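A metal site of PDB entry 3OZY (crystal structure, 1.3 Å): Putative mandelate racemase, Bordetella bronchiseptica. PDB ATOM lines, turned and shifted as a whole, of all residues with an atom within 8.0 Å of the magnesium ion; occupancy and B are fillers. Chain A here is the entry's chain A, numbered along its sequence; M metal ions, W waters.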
ATOM      1  N   SER A  25      -4.258 -21.225 -19.401  1.00  0.00           N
ATOM      2  CA  SER A  25      -4.713 -21.414 -18.032  1.00  0.00           C
ATOM      3  C   SER A  25      -5.768 -22.506 -18.077  1.00  0.00           C
ATOM      4  O   SER A  25      -6.018 -23.115 -19.125  1.00  0.00           O
ATOM      5  CB  SER A  25      -5.346 -20.135 -17.506  1.00  0.00           C
ATOM      6  OG  SER A  25      -6.544 -19.845 -18.191  1.00  0.00           O
ATOM      7  N   ALA A  27      -8.735 -22.128 -18.333  1.00  0.00           N
ATOM      8  CA  ALA A  27      -9.754 -21.734 -19.300  1.00  0.00           C
ATOM      9  C   ALA A  27      -9.411 -22.134 -20.733  1.00  0.00           C
ATOM     10  O   ALA A  27     -10.270 -22.062 -21.602  1.00  0.00           O
ATOM     11  CB  ALA A  27      -9.992 -20.240 -19.229  1.00  0.00           C
ATOM     12  N   TYR A 142      -3.728  -4.584 -10.379  1.00  0.00           N
ATOM     13  CA  TYR A 142      -2.824  -5.720 -10.395  1.00  0.00           C
ATOM     14  C   TYR A 142      -2.643  -6.218 -11.816  1.00  0.00           C
ATOM     15  O   TYR A 142      -3.542  -6.123 -12.640  1.00  0.00           O
ATOM     16  CB  TYR A 142      -3.311  -6.848  -9.475  1.00  0.00           C
ATOM     17  CG  TYR A 142      -4.500  -7.679  -9.926  1.00  0.00           C
ATOM     18  CD1 TYR A 142      -4.337  -8.781 -10.755  1.00  0.00           C
ATOM     19  CD2 TYR A 142      -5.787  -7.426  -9.420  1.00  0.00           C
ATOM     20  CE1 TYR A 142      -5.408  -9.589 -11.121  1.00  0.00           C
ATOM     21  CE2 TYR A 142      -6.867  -8.212  -9.791  1.00  0.00           C
ATOM     22  CZ  TYR A 142      -6.683  -9.298 -10.632  1.00  0.00           C
ATOM     23  OH  TYR A 142      -7.744 -10.115 -10.992  1.00  0.00           O
ATOM     24  N   SER A 144      -2.560  -8.803 -14.570  1.00  0.00           N
ATOM     25  CA  SER A 144      -3.273 -10.048 -14.812  1.00  0.00           C
ATOM     26  C   SER A 144      -2.855 -10.615 -16.179  1.00  0.00           C
ATOM     27  O   SER A 144      -3.148 -10.001 -17.199  1.00  0.00           O
ATOM     28  CB  SER A 144      -4.777  -9.753 -14.820  1.00  0.00           C
ATOM     29  OG  SER A 144      -5.531 -10.928 -14.990  1.00  0.00           O
ATOM     30  N   SER A 145      -2.150 -11.755 -16.243  1.00  0.00           N
ATOM     31  CA  SER A 145      -1.593 -12.543 -15.139  1.00  0.00           C
ATOM     32  C   SER A 145      -0.315 -13.187 -15.659  1.00  0.00           C
ATOM     33  O   SER A 145      -0.016 -13.104 -16.846  1.00  0.00           O
ATOM     34  CB  SER A 145      -2.538 -13.686 -14.753  1.00  0.00           C
ATOM     35  OG  SER A 145      -3.732 -13.214 -14.138  1.00  0.00           O
ATOM     36  N   TYR A 147       1.075 -16.652 -16.488  1.00  0.00           N
ATOM     37  CA  TYR A 147       0.345 -17.857 -16.875  1.00  0.00           C
ATOM     38  C   TYR A 147       1.140 -19.150 -16.643  1.00  0.00           C
ATOM     39  O   TYR A 147       2.218 -19.135 -16.043  1.00  0.00           O
ATOM     40  CB  TYR A 147      -0.159 -17.737 -18.335  1.00  0.00           C
ATOM     41  CG  TYR A 147      -1.470 -16.957 -18.425  1.00  0.00           C
ATOM     42  CD1 TYR A 147      -1.493 -15.578 -18.228  1.00  0.00           C
ATOM     43  CD2 TYR A 147      -2.669 -17.599 -18.681  1.00  0.00           C
ATOM     44  CE1 TYR A 147      -2.685 -14.846 -18.293  1.00  0.00           C
ATOM     45  CE2 TYR A 147      -3.872 -16.876 -18.740  1.00  0.00           C
ATOM     46  CZ  TYR A 147      -3.865 -15.517 -18.552  1.00  0.00           C
ATOM     47  OH  TYR A 147      -5.048 -14.793 -18.611  1.00  0.00           O
ATOM     48  N   LYS A 171      -1.073 -11.418 -10.445  1.00  0.00           N
ATOM     49  CA  LYS A 171      -1.746 -12.699 -10.306  1.00  0.00           C
ATOM     50  C   LYS A 171      -1.034 -13.806 -11.064  1.00  0.00           C
ATOM     51  O   LYS A 171      -0.534 -13.601 -12.181  1.00  0.00           O
ATOM     52  CB  LYS A 171      -3.203 -12.567 -10.769  1.00  0.00           C
ATOM     53  CG  LYS A 171      -4.098 -13.783 -10.491  1.00  0.00           C
ATOM     54  CD  LYS A 171      -5.581 -13.418 -10.489  1.00  0.00           C
ATOM     55  CE  LYS A 171      -6.157 -13.354 -11.894  1.00  0.00           C
ATOM     56  NZ  LYS A 171      -7.579 -12.904 -11.844  1.00  0.00           N
ATOM     57  N   LYS A 173      -1.492 -17.778 -12.548  1.00  0.00           N
ATOM     58  CA  LYS A 173      -2.361 -18.902 -12.871  1.00  0.00           C
ATOM     59  C   LYS A 173      -1.762 -20.218 -12.383  1.00  0.00           C
ATOM     60  O   LYS A 173      -0.563 -20.468 -12.562  1.00  0.00           O
ATOM     61  CB  LYS A 173      -2.558 -18.967 -14.389  1.00  0.00           C
ATOM     62  CG  LYS A 173      -3.187 -17.736 -14.989  1.00  0.00           C
ATOM     63  CD  LYS A 173      -4.645 -17.628 -14.549  1.00  0.00           C
ATOM     64  CE  LYS A 173      -5.373 -16.543 -15.328  1.00  0.00           C
ATOM     65  NZ  LYS A 173      -6.850 -16.612 -15.118  1.00  0.00           N
ATOM     66  N   VAL A 200      -3.557 -15.651  -6.695  1.00  0.00           N
ATOM     67  CA  VAL A 200      -3.481 -16.931  -7.399  1.00  0.00           C
ATOM     68  C   VAL A 200      -4.856 -17.271  -7.977  1.00  0.00           C
ATOM     69  O   VAL A 200      -5.883 -16.939  -7.354  1.00  0.00           O
ATOM     70  CB  VAL A 200      -3.008 -18.029  -6.422  1.00  0.00           C
ATOM     71  CG1 VAL A 200      -3.217 -19.413  -6.997  1.00  0.00           C
ATOM     72  CG2 VAL A 200      -1.541 -17.816  -6.036  1.00  0.00           C
ATOM     73  N   ASP A 201      -4.884 -17.897  -9.149  1.00  0.00           N
ATOM     74  CA  ASP A 201      -6.125 -18.180  -9.859  1.00  0.00           C
ATOM     75  C   ASP A 201      -6.022 -19.562 -10.497  1.00  0.00           C
ATOM     76  O   ASP A 201      -5.177 -19.772 -11.379  1.00  0.00           O
ATOM     77  CB  ASP A 201      -6.336 -17.091 -10.916  1.00  0.00           C
ATOM     78  CG  ASP A 201      -7.622 -17.262 -11.712  1.00  0.00           C
ATOM     79  OD1 ASP A 201      -8.289 -18.304 -11.606  1.00  0.00           O
ATOM     80  OD2 ASP A 201      -7.923 -16.316 -12.483  1.00  0.00           O
ATOM     81  N   ALA A 202      -6.864 -20.494 -10.046  1.00  0.00           N
ATOM     82  CA  ALA A 202      -6.826 -21.868 -10.514  1.00  0.00           C
ATOM     83  C   ALA A 202      -7.807 -22.173 -11.648  1.00  0.00           C
ATOM     84  O   ALA A 202      -7.832 -23.286 -12.140  1.00  0.00           O
ATOM     85  CB  ALA A 202      -7.065 -22.847  -9.355  1.00  0.00           C
ATOM     86  N   ASN A 203      -8.626 -21.199 -12.050  1.00  0.00           N
ATOM     87  CA  ASN A 203      -9.587 -21.432 -13.139  1.00  0.00           C
ATOM     88  C   ASN A 203     -10.401 -22.715 -12.960  1.00  0.00           C
ATOM     89  O   ASN A 203     -10.627 -23.455 -13.931  1.00  0.00           O
ATOM     90  CB  ASN A 203      -8.886 -21.427 -14.504  1.00  0.00           C
ATOM     91  CG  ASN A 203      -8.503 -20.042 -14.965  1.00  0.00           C
ATOM     92  OD1 ASN A 203      -7.378 -19.589 -14.728  1.00  0.00           O
ATOM     93  ND2 ASN A 203      -9.433 -19.361 -15.622  1.00  0.00           N
ATOM     94  N   GLN A 204     -10.836 -22.972 -11.728  1.00  0.00           N
ATOM     95  CA  GLN A 204     -11.709 -24.113 -11.419  1.00  0.00           C
ATOM     96  C   GLN A 204     -11.036 -25.472 -11.604  1.00  0.00           C
ATOM     97  O   GLN A 204     -11.716 -26.479 -11.765  1.00  0.00           O
ATOM     98  CB  GLN A 204     -12.991 -24.101 -12.256  1.00  0.00           C
ATOM     99  CG  GLN A 204     -13.740 -22.782 -12.306  1.00  0.00           C
ATOM    100  CD  GLN A 204     -15.056 -22.918 -13.092  1.00  0.00           C
ATOM    101  OE1 GLN A 204     -15.913 -23.729 -12.747  1.00  0.00           O
ATOM    102  NE2 GLN A 204     -15.203 -22.123 -14.149  1.00  0.00           N
ATOM    103  N   TRP A 225      -5.336 -13.554  -2.435  1.00  0.00           N
ATOM    104  CA  TRP A 225      -6.540 -14.341  -2.667  1.00  0.00           C
ATOM    105  C   TRP A 225      -6.260 -15.588  -3.497  1.00  0.00           C
ATOM    106  O   TRP A 225      -5.207 -15.691  -4.132  1.00  0.00           O
ATOM    107  CB  TRP A 225      -7.688 -13.508  -3.253  1.00  0.00           C
ATOM    108  CG  TRP A 225      -7.685 -13.119  -4.729  1.00  0.00           C
ATOM    109  CD1 TRP A 225      -7.338 -13.868  -5.829  1.00  0.00           C
ATOM    110  CD2 TRP A 225      -8.196 -11.881  -5.232  1.00  0.00           C
ATOM    111  NE1 TRP A 225      -7.555 -13.137  -6.988  1.00  0.00           N
ATOM    112  CE2 TRP A 225      -8.094 -11.915  -6.646  1.00  0.00           C
ATOM    113  CE3 TRP A 225      -8.713 -10.736  -4.628  1.00  0.00           C
ATOM    114  CZ2 TRP A 225      -8.492 -10.841  -7.453  1.00  0.00           C
ATOM    115  CZ3 TRP A 225      -9.111  -9.670  -5.429  1.00  0.00           C
ATOM    116  CH2 TRP A 225      -9.001  -9.735  -6.818  1.00  0.00           C
ATOM    117  N   GLU A 227      -8.352 -17.520  -6.273  1.00  0.00           N
ATOM    118  CA  GLU A 227      -9.467 -17.280  -7.184  1.00  0.00           C
ATOM    119  C   GLU A 227      -9.849 -18.551  -7.948  1.00  0.00           C
ATOM    120  O   GLU A 227      -8.976 -19.311  -8.380  1.00  0.00           O
ATOM    121  CB  GLU A 227      -9.079 -16.165  -8.157  1.00  0.00           C
ATOM    122  CG  GLU A 227     -10.008 -15.981  -9.327  1.00  0.00           C
ATOM    123  CD  GLU A 227      -9.691 -14.731 -10.114  1.00  0.00           C
ATOM    124  OE1 GLU A 227      -8.863 -13.916  -9.653  1.00  0.00           O
ATOM    125  OE2 GLU A 227     -10.273 -14.550 -11.204  1.00  0.00           O
ATOM    126  N   GLU A 228     -11.161 -18.766  -8.116  1.00  0.00           N
ATOM    127  CA  GLU A 228     -11.705 -19.982  -8.721  1.00  0.00           C
ATOM    128  C   GLU A 228     -10.913 -21.228  -8.312  1.00  0.00           C
ATOM    129  O   GLU A 228     -10.431 -21.993  -9.146  1.00  0.00           O
ATOM    130  CB  GLU A 228     -11.808 -19.869 -10.250  1.00  0.00           C
ATOM    131  CG  GLU A 228     -12.906 -18.904 -10.710  1.00  0.00           C
ATOM    132  CD  GLU A 228     -13.309 -19.160 -12.144  1.00  0.00           C
ATOM    133  OE1 GLU A 228     -12.440 -19.558 -12.957  1.00  0.00           O
ATOM    134  OE2 GLU A 228     -14.498 -18.973 -12.472  1.00  0.00           O
ATOM    135  N   ALA A 251     -11.848 -16.221  -3.465  1.00  0.00           N
ATOM    136  CA  ALA A 251     -12.425 -15.345  -4.473  1.00  0.00           C
ATOM    137  C   ALA A 251     -13.018 -16.133  -5.623  1.00  0.00           C
ATOM    138  O   ALA A 251     -12.430 -17.114  -6.076  1.00  0.00           O
ATOM    139  CB  ALA A 251     -11.331 -14.406  -5.016  1.00  0.00           C
ATOM    140  N   THR A 252     -14.177 -15.705  -6.111  1.00  0.00           N
ATOM    141  CA  THR A 252     -14.743 -16.265  -7.324  1.00  0.00           C
ATOM    142  C   THR A 252     -15.779 -15.304  -7.870  1.00  0.00           C
ATOM    143  O   THR A 252     -16.285 -14.438  -7.151  1.00  0.00           O
ATOM    144  CB  THR A 252     -15.331 -17.680  -7.093  1.00  0.00           C
ATOM    145  OG1 THR A 252     -15.696 -18.251  -8.359  1.00  0.00           O
ATOM    146  CG2 THR A 252     -16.553 -17.656  -6.144  1.00  0.00           C
ATOM    147  N   GLY A 253     -16.072 -15.417  -9.161  1.00  0.00           N
ATOM    148  CA  GLY A 253     -17.183 -14.662  -9.699  1.00  0.00           C
ATOM    149  C   GLY A 253     -17.234 -14.419 -11.188  1.00  0.00           C
ATOM    150  O   GLY A 253     -18.305 -14.061 -11.697  1.00  0.00           O
ATOM    151  N   GLU A 254     -16.141 -14.597 -11.917  1.00  0.00           N
ATOM    152  CA  GLU A 254     -16.193 -14.348 -13.349  1.00  0.00           C
ATOM    153  C   GLU A 254     -17.169 -15.285 -14.057  1.00  0.00           C
ATOM    154  O   GLU A 254     -17.687 -14.960 -15.120  1.00  0.00           O
ATOM    155  CB  GLU A 254     -14.818 -14.399 -13.997  1.00  0.00           C
ATOM    156  CG  GLU A 254     -14.295 -15.793 -14.220  1.00  0.00           C
ATOM    157  CD  GLU A 254     -12.818 -15.773 -14.493  1.00  0.00           C
ATOM    158  OE1 GLU A 254     -12.396 -16.296 -15.540  1.00  0.00           O
ATOM    159  OE2 GLU A 254     -12.094 -15.218 -13.654  1.00  0.00           O
ATOM    160  N   ASN A 255     -17.419 -16.453 -13.472  1.00  0.00           N
ATOM    161  CA  ASN A 255     -18.288 -17.438 -14.105  1.00  0.00           C
ATOM    162  C   ASN A 255     -19.591 -17.687 -13.350  1.00  0.00           C
ATOM    163  O   ASN A 255     -20.297 -18.649 -13.635  1.00  0.00           O
ATOM    164  CB  ASN A 255     -17.501 -18.723 -14.385  1.00  0.00           C
ATOM    165  CG  ASN A 255     -16.510 -18.534 -15.512  1.00  0.00           C
ATOM    166  OD1 ASN A 255     -16.875 -18.072 -16.603  1.00  0.00           O
ATOM    167  ND2 ASN A 255     -15.242 -18.842 -15.255  1.00  0.00           N
ATOM    168  N   GLN A 275     -16.383 -11.513  -7.363  1.00  0.00           N
ATOM    169  CA  GLN A 275     -15.694 -11.003  -8.550  1.00  0.00           C
ATOM    170  C   GLN A 275     -16.612 -10.760  -9.740  1.00  0.00           C
ATOM    171  O   GLN A 275     -16.175 -10.729 -10.887  1.00  0.00           O
ATOM    172  CB  GLN A 275     -14.537 -11.928  -8.917  1.00  0.00           C
ATOM    173  CG  GLN A 275     -13.505 -12.071  -7.803  1.00  0.00           C
ATOM    174  CD  GLN A 275     -12.343 -12.914  -8.245  1.00  0.00           C
ATOM    175  OE1 GLN A 275     -12.505 -14.103  -8.516  1.00  0.00           O
ATOM    176  NE2 GLN A 275     -11.167 -12.307  -8.330  1.00  0.00           N
ATOM    177  N   HIS A 304     -13.750  -9.221 -11.737  1.00  0.00           N
ATOM    178  CA  HIS A 304     -13.052  -9.652 -12.930  1.00  0.00           C
ATOM    179  C   HIS A 304     -13.303  -8.600 -14.021  1.00  0.00           C
ATOM    180  O   HIS A 304     -14.409  -8.041 -14.092  1.00  0.00           O
ATOM    181  CB  HIS A 304     -13.635 -11.014 -13.333  1.00  0.00           C
ATOM    182  CG  HIS A 304     -13.215 -11.489 -14.696  1.00  0.00           C
ATOM    183  ND1 HIS A 304     -13.839 -11.078 -15.850  1.00  0.00           N
ATOM    184  CD2 HIS A 304     -12.266 -12.373 -15.070  1.00  0.00           C
ATOM    185  CE1 HIS A 304     -13.269 -11.676 -16.889  1.00  0.00           C
ATOM    186  NE2 HIS A 304     -12.317 -12.466 -16.438  1.00  0.00           N
ATOM    187  N   THR A 305     -12.288  -8.303 -14.827  1.00  0.00           N
ATOM    188  CA  THR A 305     -12.410  -7.268 -15.867  1.00  0.00           C
ATOM    189  C   THR A 305     -11.839  -7.705 -17.220  1.00  0.00           C
ATOM    190  O   THR A 305     -11.840  -6.926 -18.176  1.00  0.00           O
ATOM    191  CB  THR A 305     -11.640  -6.016 -15.465  1.00  0.00           C
ATOM    192  OG1 THR A 305     -10.234  -6.303 -15.566  1.00  0.00           O
ATOM    193  CG2 THR A 305     -11.972  -5.571 -14.055  1.00  0.00           C
ATOM    194  N   PHE A 306     -11.386  -8.951 -17.304  1.00  0.00           N
ATOM    195  CA  PHE A 306     -10.482  -9.403 -18.366  1.00  0.00           C
ATOM    196  C   PHE A 306     -11.232  -9.785 -19.653  1.00  0.00           C
ATOM    197  O   PHE A 306     -11.865 -10.834 -19.719  1.00  0.00           O
ATOM    198  CB  PHE A 306      -9.732 -10.609 -17.809  1.00  0.00           C
ATOM    199  CG  PHE A 306      -8.503 -11.047 -18.590  1.00  0.00           C
ATOM    200  CD1 PHE A 306      -7.223 -10.669 -18.181  1.00  0.00           C
ATOM    201  CD2 PHE A 306      -8.620 -11.927 -19.654  1.00  0.00           C
ATOM    202  CE1 PHE A 306      -6.098 -11.127 -18.845  1.00  0.00           C
ATOM    203  CE2 PHE A 306      -7.494 -12.377 -20.325  1.00  0.00           C
ATOM    204  CZ  PHE A 306      -6.234 -11.971 -19.912  1.00  0.00           C
ATOM    205  N   GLU A 329      -8.245  -5.562 -11.605  1.00  0.00           N
ATOM    206  CA  GLU A 329      -7.642  -6.421 -12.619  1.00  0.00           C
ATOM    207  C   GLU A 329      -7.285  -5.664 -13.896  1.00  0.00           C
ATOM    208  O   GLU A 329      -8.127  -5.013 -14.505  1.00  0.00           O
ATOM    209  CB  GLU A 329      -8.572  -7.600 -12.951  1.00  0.00           C
ATOM    210  CG  GLU A 329      -7.971  -8.560 -13.950  1.00  0.00           C
ATOM    211  CD  GLU A 329      -8.748  -9.851 -14.107  1.00  0.00           C
ATOM    212  OE1 GLU A 329     -10.001  -9.840 -13.995  1.00  0.00           O
ATOM    213  OE2 GLU A 329      -8.116 -10.893 -14.360  1.00  0.00           O
HETATM  214 MG    MG M   1     -10.001 -15.555 -13.195  1.00  0.00          MG
HETATM  215  O   HOH W   1      -9.781 -16.425 -15.390  1.00  0.00           O
HETATM  216  O   HOH W   2     -10.518 -17.693 -12.847  1.00  0.00           O
HETATM  217  O   HOH W   3      -9.163 -13.559 -14.151  1.00  0.00           O
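Residues that only touch the magnesium ion: Lys 171 (3.8 Å) and Lys 173 (3.8 Å).
Five residues have an atom within 4 Å of the magnesium ion: Lys 171, Lys 173, Asp 201, Glu 227 and Glu 254.
The nearest printed residue that does not touch the magnesium ion is His 304 (4.3 Å).
Water W2 lies within hydrogen-bond range of OD1 of Asp 201 (2.6 Å), OE1 of Glu 228 (2.7 Å) and ND2 of Asn 203 (3.4 Å).
Water W1 lies within hydrogen-bond range of the side-chain carboxylate (OE1) of Glu 254 (2.6 Å), the side-chain amino group (NZ) of Lys 173 (2.9 Å) and the side-chain amide nitrogen (ND2) of Asn 203 (3.0 Å).
Water W3 lies within hydrogen-bond range of OE2 of Glu 329 and NZ of Lys 171.
The magnesium ion is bound by OE2 of Glu 254 (2.2 Å), water W2 (2.2 Å), OE2 of Glu 227 (2.2 Å), OD2 of Asp 201 (2.3 Å), water W3 (2.4 Å) and water W1 (2.4 Å).
The magnesium ion has six donor atoms within binding distance.
The side-chain amino group (NZ) of Lys 171 is in salt-bridge range of the side-chain carboxylate (OE2) of Glu 329 (3.3 Å).
The backbone NH of Glu 227 is in hydrogen-bond range of the backbone carbonyl oxygen of Val 200 (2.8 Å).
The side-chain carboxylate (OD2) of Asp 201 lies close to the side-chain amino group (NZ) of Lys 171 (3.5 Å).
The side-chain carboxylate (OD1) of Asp 201 is in hydrogen-bond range of the backbone NH (N) of Asn 203 (2.9 Å).
The side-chain carboxylate of Asp 201 lies close to the side-chain amino group of Lys 173, 2.9 Å away.
OE1 of Glu 227 is in hydrogen-bond range of NE1 of Trp 225 (3.1 Å).
The side-chain carboxylate of Glu 227 is in hydrogen-bond range of the side-chain amide nitrogen of Gln 275, at 3.1 Å.
The backbone carbonyl oxygen (O) of Glu 227 sits at hydrogen-bond distance from the backbone NH (N) of Ala 202.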
